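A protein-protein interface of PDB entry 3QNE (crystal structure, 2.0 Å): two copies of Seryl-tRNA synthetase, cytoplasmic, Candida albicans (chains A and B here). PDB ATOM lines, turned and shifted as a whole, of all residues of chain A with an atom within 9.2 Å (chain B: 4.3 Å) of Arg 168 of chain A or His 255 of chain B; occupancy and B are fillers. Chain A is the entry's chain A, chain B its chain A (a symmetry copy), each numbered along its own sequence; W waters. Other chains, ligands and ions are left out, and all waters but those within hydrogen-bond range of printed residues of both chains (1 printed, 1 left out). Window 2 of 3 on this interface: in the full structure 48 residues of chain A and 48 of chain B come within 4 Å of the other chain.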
ATOM      1  N   LEU A 159       2.484   3.835   7.733  1.00  0.00           N
ATOM      2  CA  LEU A 159       2.262   3.804   6.293  1.00  0.00           C
ATOM      3  C   LEU A 159       1.067   4.660   5.868  1.00  0.00           C
ATOM      4  O   LEU A 159       1.151   5.409   4.902  1.00  0.00           O
ATOM      5  CB  LEU A 159       2.023   2.370   5.833  1.00  0.00           C
ATOM      6  CG  LEU A 159       2.566   1.945   4.482  1.00  0.00           C
ATOM      7  CD1 LEU A 159       4.049   2.327   4.361  1.00  0.00           C
ATOM      8  CD2 LEU A 159       2.367   0.437   4.317  1.00  0.00           C
ATOM      9  N   ASP A 162       1.687   8.185   5.699  1.00  0.00           N
ATOM     10  CA  ASP A 162       2.808   8.511   4.815  1.00  0.00           C
ATOM     11  C   ASP A 162       3.974   9.064   5.636  1.00  0.00           C
ATOM     12  O   ASP A 162       4.572  10.075   5.267  1.00  0.00           O
ATOM     13  CB  ASP A 162       2.378   9.571   3.800  1.00  0.00           C
ATOM     14  CG  ASP A 162       3.351   9.717   2.656  1.00  0.00           C
ATOM     15  OD1 ASP A 162       4.072   8.746   2.349  1.00  0.00           O
ATOM     16  OD2 ASP A 162       3.378  10.809   2.053  1.00  0.00           O
ATOM     17  N   TYR A 164       6.734   7.209   6.759  1.00  0.00           N
ATOM     18  CA  TYR A 164       8.037   6.576   6.545  1.00  0.00           C
ATOM     19  C   TYR A 164       8.038   5.770   5.257  1.00  0.00           C
ATOM     20  O   TYR A 164       6.972   5.525   4.659  1.00  0.00           O
ATOM     21  CB  TYR A 164       8.473   5.735   7.768  1.00  0.00           C
ATOM     22  CG  TYR A 164       8.098   4.260   7.759  1.00  0.00           C
ATOM     23  CD1 TYR A 164       9.067   3.286   8.023  1.00  0.00           C
ATOM     24  CD2 TYR A 164       6.782   3.834   7.541  1.00  0.00           C
ATOM     25  CE1 TYR A 164       8.756   1.935   8.056  1.00  0.00           C
ATOM     26  CE2 TYR A 164       6.458   2.457   7.566  1.00  0.00           C
ATOM     27  CZ  TYR A 164       7.458   1.526   7.823  1.00  0.00           C
ATOM     28  OH  TYR A 164       7.182   0.180   7.865  1.00  0.00           O
ATOM     29  N   ASP A 165       9.232   5.398   4.808  1.00  0.00           N
ATOM     30  CA  ASP A 165       9.373   4.649   3.574  1.00  0.00           C
ATOM     31  C   ASP A 165      10.294   3.449   3.749  1.00  0.00           C
ATOM     32  O   ASP A 165      11.510   3.550   3.542  1.00  0.00           O
ATOM     33  CB  ASP A 165       9.946   5.520   2.466  1.00  0.00           C
ATOM     34  CG  ASP A 165       9.538   5.033   1.095  1.00  0.00           C
ATOM     35  OD1 ASP A 165       9.513   3.780   0.841  1.00  0.00           O
ATOM     36  OD2 ASP A 165       9.207   5.915   0.283  1.00  0.00           O
ATOM     37  N   PRO A 166       9.718   2.297   4.098  1.00  0.00           N
ATOM     38  CA  PRO A 166      10.544   1.096   4.236  1.00  0.00           C
ATOM     39  C   PRO A 166      10.944   0.528   2.889  1.00  0.00           C
ATOM     40  O   PRO A 166      11.996  -0.103   2.822  1.00  0.00           O
ATOM     41  CB  PRO A 166       9.623   0.103   4.991  1.00  0.00           C
ATOM     42  CG  PRO A 166       8.241   0.536   4.613  1.00  0.00           C
ATOM     43  CD  PRO A 166       8.305   2.059   4.445  1.00  0.00           C
ATOM     44  N   GLU A 167      10.138   0.728   1.841  1.00  0.00           N
ATOM     45  CA  GLU A 167      10.464   0.115   0.554  1.00  0.00           C
ATOM     46  C   GLU A 167      11.687   0.759  -0.093  1.00  0.00           C
ATOM     47  O   GLU A 167      12.624   0.075  -0.494  1.00  0.00           O
ATOM     48  CB  GLU A 167       9.274   0.112  -0.426  1.00  0.00           C
ATOM     49  CG  GLU A 167       9.662  -0.428  -1.811  1.00  0.00           C
ATOM     50  CD  GLU A 167       8.464  -0.788  -2.704  1.00  0.00           C
ATOM     51  OE1 GLU A 167       8.690  -1.030  -3.914  1.00  0.00           O
ATOM     52  OE2 GLU A 167       7.314  -0.839  -2.201  1.00  0.00           O
ATOM     53  N   ARG A 168      11.679   2.079  -0.200  1.00  0.00           N
ATOM     54  CA  ARG A 168      12.841   2.772  -0.721  1.00  0.00           C
ATOM     55  C   ARG A 168      14.029   2.649   0.265  1.00  0.00           C
ATOM     56  O   ARG A 168      15.186   2.591  -0.137  1.00  0.00           O
ATOM     57  CB  ARG A 168      12.483   4.238  -0.989  1.00  0.00           C
ATOM     58  CG  ARG A 168      11.340   4.386  -2.023  1.00  0.00           C
ATOM     59  CD  ARG A 168      11.060   5.844  -2.315  1.00  0.00           C
ATOM     60  NE  ARG A 168      10.186   6.050  -3.470  1.00  0.00           N
ATOM     61  CZ  ARG A 168       8.886   6.312  -3.384  1.00  0.00           C
ATOM     62  NH1 ARG A 168       8.306   6.386  -2.187  1.00  0.00           N
ATOM     63  NH2 ARG A 168       8.166   6.523  -4.486  1.00  0.00           N
ATOM     64  N   GLY A 169      13.728   2.584   1.554  1.00  0.00           N
ATOM     65  CA  GLY A 169      14.761   2.403   2.567  1.00  0.00           C
ATOM     66  C   GLY A 169      15.510   1.095   2.342  1.00  0.00           C
ATOM     67  O   GLY A 169      16.747   1.069   2.302  1.00  0.00           O
ATOM     68  N   VAL A 170      14.767   0.002   2.169  1.00  0.00           N
ATOM     69  CA  VAL A 170      15.415  -1.293   1.954  1.00  0.00           C
ATOM     70  C   VAL A 170      16.261  -1.278   0.681  1.00  0.00           C
ATOM     71  O   VAL A 170      17.349  -1.835   0.660  1.00  0.00           O
ATOM     72  CB  VAL A 170      14.415  -2.475   1.933  1.00  0.00           C
ATOM     73  CG1 VAL A 170      15.085  -3.742   1.393  1.00  0.00           C
ATOM     74  CG2 VAL A 170      13.862  -2.718   3.339  1.00  0.00           C
ATOM     75  N   ARG A 171      15.770  -0.626  -0.371  1.00  0.00           N
ATOM     76  CA  ARG A 171      16.523  -0.579  -1.618  1.00  0.00           C
ATOM     77  C   ARG A 171      17.873   0.088  -1.417  1.00  0.00           C
ATOM     78  O   ARG A 171      18.871  -0.361  -1.962  1.00  0.00           O
ATOM     79  CB  ARG A 171      15.761   0.170  -2.701  1.00  0.00           C
ATOM     80  CG  ARG A 171      16.435   0.066  -4.066  1.00  0.00           C
ATOM     81  CD  ARG A 171      15.510   0.564  -5.186  1.00  0.00           C
ATOM     82  NE  ARG A 171      14.774   1.771  -4.805  1.00  0.00           N
ATOM     83  CZ  ARG A 171      15.314   2.988  -4.671  1.00  0.00           C
ATOM     84  NH1 ARG A 171      16.618   3.197  -4.890  1.00  0.00           N
ATOM     85  NH2 ARG A 171      14.536   4.007  -4.312  1.00  0.00           N
ATOM     86  N   ILE A 172      17.893   1.165  -0.631  1.00  0.00           N
ATOM     87  CA  ILE A 172      19.100   1.956  -0.477  1.00  0.00           C
ATOM     88  C   ILE A 172      20.129   1.438   0.541  1.00  0.00           C
ATOM     89  O   ILE A 172      21.342   1.557   0.318  1.00  0.00           O
ATOM     90  CB  ILE A 172      18.718   3.437  -0.246  1.00  0.00           C
ATOM     91  CG1 ILE A 172      18.347   4.043  -1.616  1.00  0.00           C
ATOM     92  CG2 ILE A 172      19.853   4.186   0.394  1.00  0.00           C
ATOM     93  CD1 ILE A 172      17.286   5.116  -1.592  1.00  0.00           C
ATOM     94  N   VAL A 173      19.667   0.847   1.643  1.00  0.00           N
ATOM     95  CA  VAL A 173      20.607   0.405   2.679  1.00  0.00           C
ATOM     96  C   VAL A 173      20.392  -1.037   3.136  1.00  0.00           C
ATOM     97  O   VAL A 173      21.103  -1.523   4.002  1.00  0.00           O
ATOM     98  CB  VAL A 173      20.608   1.363   3.908  1.00  0.00           C
ATOM     99  CG1 VAL A 173      19.254   1.416   4.551  1.00  0.00           C
ATOM    100  CG2 VAL A 173      21.648   0.942   4.936  1.00  0.00           C
ATOM    101  N   GLY A 174      19.420  -1.726   2.549  1.00  0.00           N
ATOM    102  CA  GLY A 174      19.225  -3.130   2.871  1.00  0.00           C
ATOM    103  C   GLY A 174      18.323  -3.357   4.075  1.00  0.00           C
ATOM    104  O   GLY A 174      17.447  -2.540   4.388  1.00  0.00           O
ATOM    105  N   ARG A 176      15.847  -3.804   6.869  1.00  0.00           N
ATOM    106  CA  ARG A 176      15.200  -2.902   7.835  1.00  0.00           C
ATOM    107  C   ARG A 176      15.511  -1.425   7.569  1.00  0.00           C
ATOM    108  O   ARG A 176      15.285  -0.577   8.439  1.00  0.00           O
ATOM    109  CB  ARG A 176      15.631  -3.207   9.272  1.00  0.00           C
ATOM    110  CG  ARG A 176      15.468  -4.653   9.718  1.00  0.00           C
ATOM    111  CD  ARG A 176      14.022  -5.001  10.005  1.00  0.00           C
ATOM    112  NE  ARG A 176      13.893  -6.413  10.369  1.00  0.00           N
ATOM    113  CZ  ARG A 176      13.660  -6.860  11.602  1.00  0.00           C
ATOM    114  NH1 ARG A 176      13.511  -6.007  12.609  1.00  0.00           N
ATOM    115  NH2 ARG A 176      13.566  -8.168  11.827  1.00  0.00           N
ATOM    116  N   GLY A 177      16.061  -1.116   6.402  1.00  0.00           N
ATOM    117  CA  GLY A 177      16.338   0.282   6.080  1.00  0.00           C
ATOM    118  C   GLY A 177      15.076   1.122   5.980  1.00  0.00           C
ATOM    119  O   GLY A 177      14.049   0.613   5.585  1.00  0.00           O
ATOM    120  N   TYR A 178      15.149   2.414   6.312  1.00  0.00           N
ATOM    121  CA  TYR A 178      13.964   3.265   6.222  1.00  0.00           C
ATOM    122  C   TYR A 178      14.320   4.738   6.109  1.00  0.00           C
ATOM    123  O   TYR A 178      15.363   5.182   6.616  1.00  0.00           O
ATOM    124  CB  TYR A 178      13.041   3.041   7.446  1.00  0.00           C
ATOM    125  CG  TYR A 178      13.653   3.493   8.766  1.00  0.00           C
ATOM    126  CD1 TYR A 178      13.358   4.736   9.296  1.00  0.00           C
ATOM    127  CD2 TYR A 178      14.515   2.653   9.490  1.00  0.00           C
ATOM    128  CE1 TYR A 178      13.919   5.163  10.516  1.00  0.00           C
ATOM    129  CE2 TYR A 178      15.097   3.073  10.687  1.00  0.00           C
ATOM    130  CZ  TYR A 178      14.795   4.329  11.196  1.00  0.00           C
ATOM    131  OH  TYR A 178      15.364   4.751  12.383  1.00  0.00           O
ATOM    132  N   PHE A 179      13.464   5.491   5.426  1.00  0.00           N
ATOM    133  CA  PHE A 179      13.473   6.946   5.580  1.00  0.00           C
ATOM    134  C   PHE A 179      12.305   7.294   6.486  1.00  0.00           C
ATOM    135  O   PHE A 179      11.295   6.597   6.467  1.00  0.00           O
ATOM    136  CB  PHE A 179      13.185   7.622   4.248  1.00  0.00           C
ATOM    137  CG  PHE A 179      14.287   7.494   3.229  1.00  0.00           C
ATOM    138  CD1 PHE A 179      15.029   8.614   2.862  1.00  0.00           C
ATOM    139  CD2 PHE A 179      14.550   6.271   2.610  1.00  0.00           C
ATOM    140  CE1 PHE A 179      16.040   8.518   1.883  1.00  0.00           C
ATOM    141  CE2 PHE A 179      15.555   6.155   1.634  1.00  0.00           C
ATOM    142  CZ  PHE A 179      16.295   7.273   1.266  1.00  0.00           C
ATOM    143  N   LEU A 180      12.409   8.388   7.234  1.00  0.00           N
ATOM    144  CA  LEU A 180      11.227   8.991   7.861  1.00  0.00           C
ATOM    145  C   LEU A 180      10.758  10.093   6.915  1.00  0.00           C
ATOM    146  O   LEU A 180      11.567  10.684   6.221  1.00  0.00           O
ATOM    147  CB  LEU A 180      11.575   9.588   9.238  1.00  0.00           C
ATOM    148  CG  LEU A 180      11.983   8.546  10.283  1.00  0.00           C
ATOM    149  CD1 LEU A 180      12.392   9.236  11.607  1.00  0.00           C
ATOM    150  CD2 LEU A 180      10.835   7.531  10.540  1.00  0.00           C
ATOM    151  N   ARG A 181       9.454  10.357   6.870  1.00  0.00           N
ATOM    152  CA  ARG A 181       8.908  11.289   5.889  1.00  0.00           C
ATOM    153  C   ARG A 181       7.879  12.199   6.584  1.00  0.00           C
ATOM    154  O   ARG A 181       7.128  11.740   7.435  1.00  0.00           O
ATOM    155  CB  ARG A 181       8.277  10.467   4.724  1.00  0.00           C
ATOM    156  CG  ARG A 181       7.728  11.261   3.530  1.00  0.00           C
ATOM    157  CD  ARG A 181       6.937  10.355   2.462  1.00  0.00           C
ATOM    158  NE  ARG A 181       6.412  11.233   1.405  1.00  0.00           N
ATOM    159  CZ  ARG A 181       7.028  11.427   0.240  1.00  0.00           C
ATOM    160  NH1 ARG A 181       8.144  10.755  -0.012  1.00  0.00           N
ATOM    161  NH2 ARG A 181       6.532  12.268  -0.678  1.00  0.00           N
ATOM    162  N   LYS A 446      -3.138   7.730   3.081  1.00  0.00           N
ATOM    163  CA  LYS A 446      -3.050   6.572   2.190  1.00  0.00           C
ATOM    164  C   LYS A 446      -3.910   5.430   2.726  1.00  0.00           C
ATOM    165  O   LYS A 446      -4.019   5.246   3.944  1.00  0.00           O
ATOM    166  CB  LYS A 446      -1.596   6.070   2.123  1.00  0.00           C
ATOM    167  CG  LYS A 446      -0.650   6.885   1.239  1.00  0.00           C
ATOM    168  CD  LYS A 446       0.794   6.904   1.774  1.00  0.00           C
ATOM    169  CE  LYS A 446       1.436   5.512   1.842  1.00  0.00           C
ATOM    170  NZ  LYS A 446       2.803   5.484   2.489  1.00  0.00           N
ATOM    171  N   ALA B 253      18.949   8.875  -4.606  1.00  0.00           N
ATOM    172  CA  ALA B 253      18.556   7.535  -5.035  1.00  0.00           C
ATOM    173  C   ALA B 253      17.125   7.166  -4.614  1.00  0.00           C
ATOM    174  O   ALA B 253      16.606   6.118  -4.980  1.00  0.00           O
ATOM    175  CB  ALA B 253      19.551   6.509  -4.526  1.00  0.00           C
ATOM    176  N   TYR B 254      16.472   8.051  -3.874  1.00  0.00           N
ATOM    177  CA  TYR B 254      15.132   7.772  -3.354  1.00  0.00           C
ATOM    178  C   TYR B 254      14.166   7.358  -4.470  1.00  0.00           C
ATOM    179  O   TYR B 254      13.378   6.422  -4.310  1.00  0.00           O
ATOM    180  CB  TYR B 254      14.605   9.017  -2.648  1.00  0.00           C
ATOM    181  CG  TYR B 254      13.314   8.888  -1.849  1.00  0.00           C
ATOM    182  CD1 TYR B 254      13.279   8.222  -0.624  1.00  0.00           C
ATOM    183  CD2 TYR B 254      12.143   9.498  -2.295  1.00  0.00           C
ATOM    184  CE1 TYR B 254      12.096   8.158   0.133  1.00  0.00           C
ATOM    185  CE2 TYR B 254      10.969   9.449  -1.544  1.00  0.00           C
ATOM    186  CZ  TYR B 254      10.959   8.780  -0.336  1.00  0.00           C
ATOM    187  OH  TYR B 254       9.788   8.730   0.369  1.00  0.00           O
ATOM    188  N   HIS B 255      14.227   8.049  -5.603  1.00  0.00           N
ATOM    189  CA  HIS B 255      13.318   7.740  -6.710  1.00  0.00           C
ATOM    190  C   HIS B 255      13.990   6.901  -7.804  1.00  0.00           C
ATOM    191  O   HIS B 255      13.499   6.868  -8.936  1.00  0.00           O
ATOM    192  CB  HIS B 255      12.748   9.024  -7.320  1.00  0.00           C
ATOM    193  CG  HIS B 255      11.778   9.739  -6.432  1.00  0.00           C
ATOM    194  ND1 HIS B 255      10.547   9.209  -6.100  1.00  0.00           N
ATOM    195  CD2 HIS B 255      11.853  10.941  -5.810  1.00  0.00           C
ATOM    196  CE1 HIS B 255       9.912  10.050  -5.302  1.00  0.00           C
ATOM    197  NE2 HIS B 255      10.681  11.106  -5.105  1.00  0.00           N
ATOM    198  N   ALA B 256      15.113   6.247  -7.487  1.00  0.00           N
ATOM    199  CA  ALA B 256      15.801   5.416  -8.482  1.00  0.00           C
ATOM    200  C   ALA B 256      14.791   4.452  -9.095  1.00  0.00           C
ATOM    201  O   ALA B 256      13.960   3.887  -8.372  1.00  0.00           O
ATOM    202  CB  ALA B 256      16.961   4.613  -7.852  1.00  0.00           C
ATOM    203  N   GLY B 257      14.855   4.268 -10.409  1.00  0.00           N
ATOM    204  CA  GLY B 257      14.023   3.272 -11.078  1.00  0.00           C
ATOM    205  C   GLY B 257      12.550   3.658 -11.143  1.00  0.00           C
ATOM    206  O   GLY B 257      11.698   2.819 -11.398  1.00  0.00           O
ATOM    207  N   GLU B 258      12.254   4.934 -10.909  1.00  0.00           N
ATOM    208  CA  GLU B 258      10.880   5.428 -10.971  1.00  0.00           C
ATOM    209  C   GLU B 258      10.717   6.369 -12.162  1.00  0.00           C
ATOM    210  O   GLU B 258      11.691   6.761 -12.796  1.00  0.00           O
ATOM    211  CB  GLU B 258      10.475   6.108  -9.651  1.00  0.00           C
ATOM    212  CG  GLU B 258      10.449   5.106  -8.483  1.00  0.00           C
ATOM    213  CD  GLU B 258      10.140   5.754  -7.134  1.00  0.00           C
ATOM    214  OE1 GLU B 258       9.469   6.796  -7.101  1.00  0.00           O
ATOM    215  OE2 GLU B 258      10.569   5.207  -6.107  1.00  0.00           O
ATOM    216  N   PHE B 260       8.481   9.730 -13.589  1.00  0.00           N
ATOM    217  CA  PHE B 260       7.521  10.807 -13.510  1.00  0.00           C
ATOM    218  C   PHE B 260       6.915  11.004 -14.902  1.00  0.00           C
ATOM    219  O   PHE B 260       7.386  11.822 -15.700  1.00  0.00           O
ATOM    220  CB  PHE B 260       8.209  12.083 -12.997  1.00  0.00           C
ATOM    221  CG  PHE B 260       8.732  11.941 -11.601  1.00  0.00           C
ATOM    222  CD1 PHE B 260       7.915  12.205 -10.517  1.00  0.00           C
ATOM    223  CD2 PHE B 260      10.024  11.504 -11.376  1.00  0.00           C
ATOM    224  CE1 PHE B 260       8.381  12.057  -9.234  1.00  0.00           C
ATOM    225  CE2 PHE B 260      10.503  11.367 -10.093  1.00  0.00           C
ATOM    226  CZ  PHE B 260       9.677  11.637  -9.021  1.00  0.00           C
ATOM    227  N   VAL B 269       9.511  17.903  -7.546  1.00  0.00           N
ATOM    228  CA  VAL B 269       9.419  17.310  -6.227  1.00  0.00           C
ATOM    229  C   VAL B 269      10.575  17.881  -5.407  1.00  0.00           C
ATOM    230  O   VAL B 269      11.725  17.858  -5.858  1.00  0.00           O
ATOM    231  CB  VAL B 269       9.500  15.778  -6.302  1.00  0.00           C
ATOM    232  CG1 VAL B 269       9.860  15.231  -4.965  1.00  0.00           C
ATOM    233  CG2 VAL B 269       8.146  15.219  -6.751  1.00  0.00           C
ATOM    234  N   TYR B 271      12.547  18.058  -1.639  1.00  0.00           N
ATOM    235  CA  TYR B 271      12.765  17.426  -0.332  1.00  0.00           C
ATOM    236  C   TYR B 271      13.671  18.263   0.563  1.00  0.00           C
ATOM    237  O   TYR B 271      14.701  18.771   0.112  1.00  0.00           O
ATOM    238  CB  TYR B 271      13.425  16.055  -0.497  1.00  0.00           C
ATOM    239  CG  TYR B 271      12.510  15.092  -1.185  1.00  0.00           C
ATOM    240  CD1 TYR B 271      11.323  14.692  -0.574  1.00  0.00           C
ATOM    241  CD2 TYR B 271      12.795  14.617  -2.459  1.00  0.00           C
ATOM    242  CE1 TYR B 271      10.445  13.806  -1.206  1.00  0.00           C
ATOM    243  CE2 TYR B 271      11.921  13.717  -3.097  1.00  0.00           C
ATOM    244  CZ  TYR B 271      10.740  13.328  -2.455  1.00  0.00           C
ATOM    245  OH  TYR B 271       9.854  12.450  -3.058  1.00  0.00           O
ATOM    246  N   LEU B 306      13.948  17.494  -7.748  1.00  0.00           N
ATOM    247  CA  LEU B 306      13.861  16.931  -9.085  1.00  0.00           C
ATOM    248  C   LEU B 306      12.921  17.808  -9.906  1.00  0.00           C
ATOM    249  O   LEU B 306      11.847  18.181  -9.428  1.00  0.00           O
ATOM    250  CB  LEU B 306      13.287  15.512  -9.011  1.00  0.00           C
ATOM    251  CG  LEU B 306      14.017  14.490  -8.144  1.00  0.00           C
ATOM    252  CD1 LEU B 306      13.418  13.106  -8.404  1.00  0.00           C
ATOM    253  CD2 LEU B 306      15.501  14.501  -8.519  1.00  0.00           C
ATOM    254  N   ILE B 383      15.885   7.578 -13.319  1.00  0.00           N
ATOM    255  CA  ILE B 383      14.744   8.373 -12.873  1.00  0.00           C
ATOM    256  C   ILE B 383      14.184   9.133 -14.071  1.00  0.00           C
ATOM    257  O   ILE B 383      14.680  10.205 -14.439  1.00  0.00           O
ATOM    258  CB  ILE B 383      15.138   9.373 -11.747  1.00  0.00           C
ATOM    259  CG1 ILE B 383      15.969   8.668 -10.664  1.00  0.00           C
ATOM    260  CG2 ILE B 383      13.884  10.018 -11.200  1.00  0.00           C
ATOM    261  CD1 ILE B 383      16.438   9.546  -9.449  1.00  0.00           C
HETATM  262  O   HOH W   1       7.163  13.850  -3.170  1.00  0.00           O
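The side-chain carboxylate (OD2) of Asp 165 of chain A is in hydrogen-bond range of the side-chain hydroxyl (OH) of Tyr 254 of chain B, 2.9 Å away.
O of Tyr 254 of chain B sits close to NE of Arg 168 of chain A (3.3 Å).
The guanidinium group (NE) of Arg 168 of chain A is in salt-bridge range of the side-chain carboxylate (OE2) of Glu 258 of chain B.
NH1 of Arg 171 of chain A is in hydrogen-bond range of O of Ala 253 of chain B (2.9 Å).
The guanidinium group of Arg 171 of chain A lies within hydrogen-bond range of the backbone carbonyl oxygen of Tyr 254 of chain B (2.7 Å).
OH of Tyr 254 of chain B is in hydrogen-bond range of NH1 of Arg 181 of chain A (2.6 Å).
NE of Arg 181 of chain A lies within salt-bridge range of OD2 of Asp 162 of chain A (3.1 Å).
N of Glu 167 of chain A sits at hydrogen-bond distance from OD1 of Asp 165 of chain A (3.3 Å).
The side-chain carboxylate (OD2) of Asp 165 of chain A lies within salt-bridge range of the guanidinium group (NH1) of Arg 168 of chain A (2.7 Å).
O of Phe 179 of chain A sits at hydrogen-bond distance from N of Asp 165 of chain A (2.9 Å).
The side-chain carboxylate of Glu 258 of chain B is in hydrogen-bond range of a ring nitrogen (ND1) of His 255 of chain B (2.8 Å).
A ring nitrogen (NE2) of His 255 of chain B lies within hydrogen-bond range of the side-chain hydroxyl (OH) of Tyr 271 of chain B (2.6 Å).
Among the printed residues, merely in contact across the chains: Arg 168 of chain A with His 255 of chain B (3.9 Å), Arg 171 of chain A with Ala 256 of chain B (3.3 Å), Ile 172 of chain A with Ala 253 of chain B (3.6 Å), Ile 172 of chain A with Tyr 254 of chain B (3.8 Å), Phe 179 of chain A with Tyr 254 of chain B (3.7 Å) and Arg 181 of chain A with Tyr 271 of chain B (3.9 Å).
Of the printed residues of chain B, Asp 165 of chain A touches Tyr 254.
Of chain B, only Tyr 254, His 255 and Glu 258 come within 4 Å of Arg 168 of chain A.
Printed residues of chain B within 4 Å of Arg 171 of chain A: Ala 253, Tyr 254 and Ala 256.
Of the printed residues of chain B, Phe 179 of chain A touches Tyr 254.
Of the printed residues of chain A, Ala 253 of chain B touches Arg 171 and Ile 172.
Tyr 254 of chain B touches just these residues of chain A: Asp 165 (2.9 Å), Arg 168 (3.1 Å), Arg 171 (2.7 Å), Ile 172 (3.8 Å), Phe 179 (3.7 Å) and Arg 181 (2.6 Å).
Of the printed residues of chain A, Ala 256 of chain B touches Arg 171 (3.3 Å).
Glu 258 of chain B touches just one residue of chain A: Arg 168 (2.8 Å).
Of the printed residues of chain A, Tyr 271 of chain B touches Arg 181 (3.9 Å).
The nearest printed residue of chain A that does not touch Ala 253 of chain B is Phe 179 of chain A (5.9 Å).
Printed residues of chain B that touch a printed residue of chain A: Ala 253, Tyr 254, His 255, Ala 256, Glu 258 and Tyr 271.
Along chain A the printed residues that touch a printed residue of chain B span positions 165 to 181.
No position is printed for both chains.
Water W1 bridges NH2 of Arg 181 of chain A (3.0 Å) and OH of Tyr 271 of chain B (3.0 Å).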
